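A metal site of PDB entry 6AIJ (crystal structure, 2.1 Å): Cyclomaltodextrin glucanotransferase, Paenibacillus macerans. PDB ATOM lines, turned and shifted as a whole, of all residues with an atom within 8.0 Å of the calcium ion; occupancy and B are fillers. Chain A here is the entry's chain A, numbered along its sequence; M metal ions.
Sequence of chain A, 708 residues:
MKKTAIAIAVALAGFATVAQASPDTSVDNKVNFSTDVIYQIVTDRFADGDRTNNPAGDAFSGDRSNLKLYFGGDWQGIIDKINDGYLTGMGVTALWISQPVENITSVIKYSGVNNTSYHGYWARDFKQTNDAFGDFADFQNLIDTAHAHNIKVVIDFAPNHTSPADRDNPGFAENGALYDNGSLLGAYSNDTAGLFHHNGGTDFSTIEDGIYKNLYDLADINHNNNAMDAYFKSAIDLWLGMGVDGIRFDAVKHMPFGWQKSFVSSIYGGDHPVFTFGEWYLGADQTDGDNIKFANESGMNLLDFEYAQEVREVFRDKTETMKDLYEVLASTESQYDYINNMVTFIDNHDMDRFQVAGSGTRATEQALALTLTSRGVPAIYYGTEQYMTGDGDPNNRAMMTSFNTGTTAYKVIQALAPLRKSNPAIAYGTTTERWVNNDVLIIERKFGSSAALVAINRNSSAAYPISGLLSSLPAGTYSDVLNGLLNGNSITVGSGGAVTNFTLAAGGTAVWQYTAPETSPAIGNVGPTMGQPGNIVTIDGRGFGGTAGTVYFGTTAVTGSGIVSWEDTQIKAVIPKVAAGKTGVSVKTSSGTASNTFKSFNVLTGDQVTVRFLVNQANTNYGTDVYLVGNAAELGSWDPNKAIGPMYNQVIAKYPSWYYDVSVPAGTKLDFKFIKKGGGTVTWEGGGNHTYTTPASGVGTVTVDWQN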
ATOM      1  N   THR A  43     -24.951 -27.054  -0.302  1.00  0.00           N
ATOM      2  CA  THR A  43     -24.895 -26.407   0.998  1.00  0.00           C
ATOM      3  C   THR A  43     -25.526 -25.023   0.997  1.00  0.00           C
ATOM      4  O   THR A  43     -26.331 -24.689   1.893  1.00  0.00           O
ATOM      5  CB  THR A  43     -23.433 -26.314   1.455  1.00  0.00           C
ATOM      6  OG1 THR A  43     -22.872 -27.640   1.519  1.00  0.00           O
ATOM      7  CG2 THR A  43     -23.320 -25.661   2.850  1.00  0.00           C
ATOM      8  N   ASP A  44     -25.184 -24.177   0.014  1.00  0.00           N
ATOM      9  CA  ASP A  44     -25.698 -22.800  -0.013  1.00  0.00           C
ATOM     10  C   ASP A  44     -27.221 -22.730  -0.176  1.00  0.00           C
ATOM     11  O   ASP A  44     -27.823 -21.682   0.117  1.00  0.00           O
ATOM     12  CB  ASP A  44     -25.036 -22.017  -1.149  1.00  0.00           C
ATOM     13  CG  ASP A  44     -25.435 -20.548  -1.150  1.00  0.00           C
ATOM     14  OD1 ASP A  44     -25.113 -19.837  -0.182  1.00  0.00           O
ATOM     15  OD2 ASP A  44     -26.060 -20.114  -2.139  1.00  0.00           O
ATOM     16  N   ALA A  47     -30.153 -24.537   4.033  1.00  0.00           N
ATOM     17  CA  ALA A  47     -30.679 -23.867   5.228  1.00  0.00           C
ATOM     18  C   ALA A  47     -29.660 -22.860   5.748  1.00  0.00           C
ATOM     19  O   ALA A  47     -28.529 -23.244   6.059  1.00  0.00           O
ATOM     20  CB  ALA A  47     -31.013 -24.888   6.344  1.00  0.00           C
ATOM     21  N   ASP A  48     -30.055 -21.595   5.868  1.00  0.00           N
ATOM     22  CA  ASP A  48     -29.176 -20.557   6.400  1.00  0.00           C
ATOM     23  C   ASP A  48     -29.343 -20.516   7.922  1.00  0.00           C
ATOM     24  O   ASP A  48     -30.252 -19.873   8.441  1.00  0.00           O
ATOM     25  CB  ASP A  48     -29.490 -19.206   5.766  1.00  0.00           C
ATOM     26  CG  ASP A  48     -28.529 -18.099   6.226  1.00  0.00           C
ATOM     27  OD1 ASP A  48     -27.654 -18.366   7.079  1.00  0.00           O
ATOM     28  OD2 ASP A  48     -28.669 -16.955   5.735  1.00  0.00           O
ATOM     29  N   GLY A  49     -28.447 -21.214   8.624  1.00  0.00           N
ATOM     30  CA  GLY A  49     -28.425 -21.251  10.063  1.00  0.00           C
ATOM     31  C   GLY A  49     -27.558 -20.209  10.737  1.00  0.00           C
ATOM     32  O   GLY A  49     -27.497 -20.161  11.965  1.00  0.00           O
ATOM     33  N   ASP A  50     -26.867 -19.368   9.956  1.00  0.00           N
ATOM     34  CA  ASP A  50     -26.002 -18.335  10.518  1.00  0.00           C
ATOM     35  C   ASP A  50     -25.897 -17.229   9.475  1.00  0.00           C
ATOM     36  O   ASP A  50     -25.154 -17.356   8.499  1.00  0.00           O
ATOM     37  CB  ASP A  50     -24.640 -18.930  10.877  1.00  0.00           C
ATOM     38  CG  ASP A  50     -23.645 -17.891  11.386  1.00  0.00           C
ATOM     39  OD1 ASP A  50     -24.035 -16.748  11.672  1.00  0.00           O
ATOM     40  OD2 ASP A  50     -22.458 -18.250  11.505  1.00  0.00           O
ATOM     41  N   ARG A  51     -26.645 -16.141   9.674  1.00  0.00           N
ATOM     42  CA  ARG A  51     -26.589 -15.025   8.740  1.00  0.00           C
ATOM     43  C   ARG A  51     -25.312 -14.207   8.840  1.00  0.00           C
ATOM     44  O   ARG A  51     -25.043 -13.416   7.925  1.00  0.00           O
ATOM     45  CB  ARG A  51     -27.805 -14.139   8.934  1.00  0.00           C
ATOM     46  CG  ARG A  51     -29.048 -14.693   8.264  1.00  0.00           C
ATOM     47  CD  ARG A  51     -30.136 -14.932   9.272  1.00  0.00           C
ATOM     48  NE  ARG A  51     -29.815 -16.025  10.192  1.00  0.00           N
ATOM     49  CZ  ARG A  51     -30.382 -16.164  11.374  1.00  0.00           C
ATOM     50  NH1 ARG A  51     -31.291 -15.285  11.776  1.00  0.00           N
ATOM     51  NH2 ARG A  51     -30.032 -17.186  12.164  1.00  0.00           N
ATOM     52  N   THR A  52     -24.503 -14.369   9.885  1.00  0.00           N
ATOM     53  CA  THR A  52     -23.278 -13.578  10.023  1.00  0.00           C
ATOM     54  C   THR A  52     -22.163 -14.028   9.092  1.00  0.00           C
ATOM     55  O   THR A  52     -21.235 -13.251   8.838  1.00  0.00           O
ATOM     56  CB  THR A  52     -22.758 -13.591  11.459  1.00  0.00           C
ATOM     57  OG1 THR A  52     -22.105 -14.848  11.725  1.00  0.00           O
ATOM     58  CG2 THR A  52     -23.871 -13.345  12.455  1.00  0.00           C
ATOM     59  N   ASN A  53     -22.204 -15.261   8.578  1.00  0.00           N
ATOM     60  CA  ASN A  53     -21.245 -15.693   7.576  1.00  0.00           C
ATOM     61  C   ASN A  53     -21.772 -15.522   6.153  1.00  0.00           C
ATOM     62  O   ASN A  53     -21.183 -16.059   5.205  1.00  0.00           O
ATOM     63  CB  ASN A  53     -20.833 -17.146   7.813  1.00  0.00           C
ATOM     64  CG  ASN A  53     -21.993 -18.137   7.660  1.00  0.00           C
ATOM     65  OD1 ASN A  53     -22.957 -17.891   6.943  1.00  0.00           O
ATOM     66  ND2 ASN A  53     -21.879 -19.277   8.314  1.00  0.00           N
ATOM     67  N   ASN A  54     -22.868 -14.794   5.993  1.00  0.00           N
ATOM     68  CA  ASN A  54     -23.449 -14.578   4.673  1.00  0.00           C
ATOM     69  C   ASN A  54     -22.577 -13.630   3.866  1.00  0.00           C
ATOM     70  O   ASN A  54     -22.273 -12.533   4.343  1.00  0.00           O
ATOM     71  CB  ASN A  54     -24.861 -14.007   4.802  1.00  0.00           C
ATOM     72  CG  ASN A  54     -25.887 -15.070   5.055  1.00  0.00           C
ATOM     73  OD1 ASN A  54     -25.545 -16.224   5.306  1.00  0.00           O
ATOM     74  ND2 ASN A  54     -27.155 -14.697   4.990  1.00  0.00           N
ATOM     75  N   PRO A  55     -22.156 -14.022   2.661  1.00  0.00           N
ATOM     76  CA  PRO A  55     -21.447 -13.068   1.777  1.00  0.00           C
ATOM     77  C   PRO A  55     -22.260 -11.805   1.545  1.00  0.00           C
ATOM     78  O   PRO A  55     -23.488 -11.819   1.556  1.00  0.00           O
ATOM     79  CB  PRO A  55     -21.276 -13.866   0.486  1.00  0.00           C
ATOM     80  CG  PRO A  55     -21.325 -15.314   0.916  1.00  0.00           C
ATOM     81  CD  PRO A  55     -22.263 -15.364   2.084  1.00  0.00           C
ATOM     82  N   PHE A  60     -24.095 -11.829  -3.054  1.00  0.00           N
ATOM     83  CA  PHE A  60     -25.241 -12.330  -2.327  1.00  0.00           C
ATOM     84  C   PHE A  60     -26.531 -11.918  -3.033  1.00  0.00           C
ATOM     85  O   PHE A  60     -26.650 -10.784  -3.514  1.00  0.00           O
ATOM     86  CB  PHE A  60     -25.239 -11.798  -0.885  1.00  0.00           C
ATOM     87  CG  PHE A  60     -26.233 -12.475   0.029  1.00  0.00           C
ATOM     88  CD1 PHE A  60     -25.884 -13.640   0.713  1.00  0.00           C
ATOM     89  CD2 PHE A  60     -27.502 -11.951   0.215  1.00  0.00           C
ATOM     90  CE1 PHE A  60     -26.792 -14.265   1.547  1.00  0.00           C
ATOM     91  CE2 PHE A  60     -28.412 -12.567   1.053  1.00  0.00           C
ATOM     92  CZ  PHE A  60     -28.052 -13.723   1.720  1.00  0.00           C
ATOM     93  N   TYR A  70     -24.544 -16.425  -3.938  1.00  0.00           N
ATOM     94  CA  TYR A  70     -24.723 -17.056  -2.642  1.00  0.00           C
ATOM     95  C   TYR A  70     -26.076 -16.701  -2.066  1.00  0.00           C
ATOM     96  O   TYR A  70     -26.445 -15.515  -2.033  1.00  0.00           O
ATOM     97  CB  TYR A  70     -23.629 -16.611  -1.682  1.00  0.00           C
ATOM     98  CG  TYR A  70     -22.307 -17.339  -1.798  1.00  0.00           C
ATOM     99  CD1 TYR A  70     -21.294 -16.858  -2.631  1.00  0.00           C
ATOM    100  CD2 TYR A  70     -22.060 -18.494  -1.063  1.00  0.00           C
ATOM    101  CE1 TYR A  70     -20.080 -17.509  -2.724  1.00  0.00           C
ATOM    102  CE2 TYR A  70     -20.845 -19.145  -1.156  1.00  0.00           C
ATOM    103  CZ  TYR A  70     -19.847 -18.647  -1.983  1.00  0.00           C
ATOM    104  OH  TYR A  70     -18.623 -19.280  -2.089  1.00  0.00           O
ATOM    105  N   PHE A  71     -26.812 -17.714  -1.614  1.00  0.00           N
ATOM    106  CA  PHE A  71     -28.083 -17.533  -0.921  1.00  0.00           C
ATOM    107  C   PHE A  71     -27.949 -17.528   0.611  1.00  0.00           C
ATOM    108  O   PHE A  71     -28.817 -16.971   1.281  1.00  0.00           O
ATOM    109  CB  PHE A  71     -29.066 -18.643  -1.307  1.00  0.00           C
ATOM    110  CG  PHE A  71     -29.730 -18.458  -2.648  1.00  0.00           C
ATOM    111  CD1 PHE A  71     -29.350 -17.452  -3.515  1.00  0.00           C
ATOM    112  CD2 PHE A  71     -30.765 -19.303  -3.033  1.00  0.00           C
ATOM    113  CE1 PHE A  71     -29.986 -17.296  -4.746  1.00  0.00           C
ATOM    114  CE2 PHE A  71     -31.392 -19.149  -4.254  1.00  0.00           C
ATOM    115  CZ  PHE A  71     -31.013 -18.147  -5.111  1.00  0.00           C
ATOM    116  N   GLY A  72     -26.926 -18.181   1.168  1.00  0.00           N
ATOM    117  CA  GLY A  72     -26.690 -18.150   2.610  1.00  0.00           C
ATOM    118  C   GLY A  72     -26.681 -19.510   3.313  1.00  0.00           C
ATOM    119  O   GLY A  72     -26.364 -19.558   4.509  1.00  0.00           O
ATOM    120  N   GLY A  73     -27.029 -20.605   2.647  1.00  0.00           N
ATOM    121  CA  GLY A  73     -27.051 -21.889   3.337  1.00  0.00           C
ATOM    122  C   GLY A  73     -25.666 -22.295   3.812  1.00  0.00           C
ATOM    123  O   GLY A  73     -24.660 -22.014   3.165  1.00  0.00           O
ATOM    124  N   ASP A  74     -25.615 -22.952   4.975  1.00  0.00           N
ATOM    125  CA  ASP A  74     -24.333 -23.184   5.615  1.00  0.00           C
ATOM    126  C   ASP A  74     -24.399 -24.429   6.481  1.00  0.00           C
ATOM    127  O   ASP A  74     -25.461 -25.055   6.647  1.00  0.00           O
ATOM    128  CB  ASP A  74     -23.906 -21.970   6.436  1.00  0.00           C
ATOM    129  CG  ASP A  74     -25.005 -21.500   7.378  1.00  0.00           C
ATOM    130  OD1 ASP A  74     -25.698 -22.342   7.973  1.00  0.00           O
ATOM    131  OD2 ASP A  74     -25.164 -20.274   7.533  1.00  0.00           O
ATOM    132  N   TRP A  75     -23.240 -24.794   7.054  1.00  0.00           N
ATOM    133  CA  TRP A  75     -23.171 -26.000   7.872  1.00  0.00           C
ATOM    134  C   TRP A  75     -24.036 -25.880   9.119  1.00  0.00           C
ATOM    135  O   TRP A  75     -24.649 -26.864   9.539  1.00  0.00           O
ATOM    136  CB  TRP A  75     -21.712 -26.309   8.231  1.00  0.00           C
ATOM    137  CG  TRP A  75     -20.881 -26.623   7.007  1.00  0.00           C
ATOM    138  CD1 TRP A  75     -21.314 -27.241   5.863  1.00  0.00           C
ATOM    139  CD2 TRP A  75     -19.496 -26.302   6.791  1.00  0.00           C
ATOM    140  NE1 TRP A  75     -20.280 -27.329   4.950  1.00  0.00           N
ATOM    141  CE2 TRP A  75     -19.153 -26.762   5.496  1.00  0.00           C
ATOM    142  CE3 TRP A  75     -18.516 -25.672   7.560  1.00  0.00           C
ATOM    143  CZ2 TRP A  75     -17.868 -26.611   4.969  1.00  0.00           C
ATOM    144  CZ3 TRP A  75     -17.231 -25.521   7.033  1.00  0.00           C
ATOM    145  CH2 TRP A  75     -16.928 -25.991   5.741  1.00  0.00           C
ATOM    146  N   GLN A  76     -24.142 -24.686   9.701  1.00  0.00           N
ATOM    147  CA  GLN A  76     -25.011 -24.518  10.859  1.00  0.00           C
ATOM    148  C   GLN A  76     -26.448 -24.910  10.549  1.00  0.00           C
ATOM    149  O   GLN A  76     -27.128 -25.533  11.370  1.00  0.00           O
ATOM    150  CB  GLN A  76     -24.960 -23.080  11.364  1.00  0.00           C
ATOM    151  CG  GLN A  76     -25.721 -22.912  12.684  1.00  0.00           C
ATOM    152  CD  GLN A  76     -25.076 -23.715  13.800  1.00  0.00           C
ATOM    153  OE1 GLN A  76     -23.943 -23.443  14.209  1.00  0.00           O
ATOM    154  NE2 GLN A  76     -25.794 -24.703  14.308  1.00  0.00           N
ATOM    155  N   GLY A  77     -26.926 -24.555   9.351  1.00  0.00           N
ATOM    156  CA  GLY A  77     -28.269 -24.931   8.946  1.00  0.00           C
ATOM    157  C   GLY A  77     -28.450 -26.436   8.828  1.00  0.00           C
ATOM    158  O   GLY A  77     -29.470 -26.974   9.232  1.00  0.00           O
ATOM    159  N   ASP A 131     -15.554 -19.909   4.035  1.00  0.00           N
ATOM    160  CA  ASP A 131     -16.114 -19.263   5.217  1.00  0.00           C
ATOM    161  C   ASP A 131     -17.615 -18.983   5.093  1.00  0.00           C
ATOM    162  O   ASP A 131     -18.266 -18.716   6.126  1.00  0.00           O
ATOM    163  CB  ASP A 131     -15.386 -17.953   5.515  1.00  0.00           C
ATOM    164  CG  ASP A 131     -13.899 -18.147   5.774  1.00  0.00           C
ATOM    165  OD1 ASP A 131     -13.450 -19.276   6.100  1.00  0.00           O
ATOM    166  OD2 ASP A 131     -13.169 -17.146   5.644  1.00  0.00           O
ATOM    167  N   ALA A 132     -18.176 -18.995   3.883  1.00  0.00           N
ATOM    168  CA  ALA A 132     -19.624 -18.912   3.754  1.00  0.00           C
ATOM    169  C   ALA A 132     -20.305 -20.091   4.423  1.00  0.00           C
ATOM    170  O   ALA A 132     -21.358 -19.937   5.057  1.00  0.00           O
ATOM    171  CB  ALA A 132     -20.025 -18.848   2.285  1.00  0.00           C
ATOM    172  N   PHE A 133     -19.726 -21.280   4.297  1.00  0.00           N
ATOM    173  CA  PHE A 133     -20.336 -22.463   4.905  1.00  0.00           C
ATOM    174  C   PHE A 133     -20.060 -22.543   6.400  1.00  0.00           C
ATOM    175  O   PHE A 133     -20.900 -23.064   7.154  1.00  0.00           O
ATOM    176  CB  PHE A 133     -19.805 -23.715   4.212  1.00  0.00           C
ATOM    177  CG  PHE A 133     -20.075 -23.750   2.732  1.00  0.00           C
ATOM    178  CD1 PHE A 133     -21.088 -22.972   2.175  1.00  0.00           C
ATOM    179  CD2 PHE A 133     -19.336 -24.569   1.905  1.00  0.00           C
ATOM    180  CE1 PHE A 133     -21.344 -23.019   0.812  1.00  0.00           C
ATOM    181  CE2 PHE A 133     -19.580 -24.623   0.540  1.00  0.00           C
ATOM    182  CZ  PHE A 133     -20.584 -23.848  -0.007  1.00  0.00           C
ATOM    183  N   GLY A 134     -18.918 -22.045   6.852  1.00  0.00           N
ATOM    184  CA  GLY A 134     -18.560 -22.034   8.252  1.00  0.00           C
ATOM    185  C   GLY A 134     -17.040 -22.010   8.400  1.00  0.00           C
ATOM    186  O   GLY A 134     -16.295 -22.028   7.428  1.00  0.00           O
HETATM  187 CA    CA M   1     -25.176 -18.367   6.280  1.00  0.00          CA
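The backbone NH (N) of Gly 49 is in hydrogen-bond range of the side-chain carboxylate (OD1) of Asp 74.
The backbone NH of Asp 74 lies within hydrogen-bond range of the backbone carbonyl oxygen of Ala 47 (3.1 Å).
The backbone NH (N) of Gln 76 lies close to the side-chain carboxylate (OD1) of Asp 74, at 3.3 Å.
OD1 of Asp 74 lies within hydrogen-bond range of N of Gly 77 (2.9 Å).
The side-chain amide nitrogen (ND2) of Asn 53 sits close to the backbone carbonyl oxygen (O) of Ala 132 (3.4 Å).
The side-chain carboxylate of Asp 50 is in hydrogen-bond range of the side-chain hydroxyl of Thr 52, at 2.7 Å.
The side-chain carboxylate of Asp 44 lies within hydrogen-bond range of the backbone NH of Gly 72 (2.8 Å).
Within 4 Å of the calcium ion: Asp 48, Asp 50, Asn 53, Asn 54, Gly 72 and Asp 74.
The nearest printed residue that does not touch the calcium ion is Ala 132 (4.3 Å).
OD2 of Asp 74 binds the calcium ion.
The calcium ion is bound by OD1 of Asn 53 (2.4 Å).
OD1 of Asn 54 is bound to the calcium ion, 2.4 Å away.
O of Asp 50 is bound to the calcium ion.
The calcium ion is bound by O of Gly 72.
The calcium ion is bound by OD1 of Asp 48.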
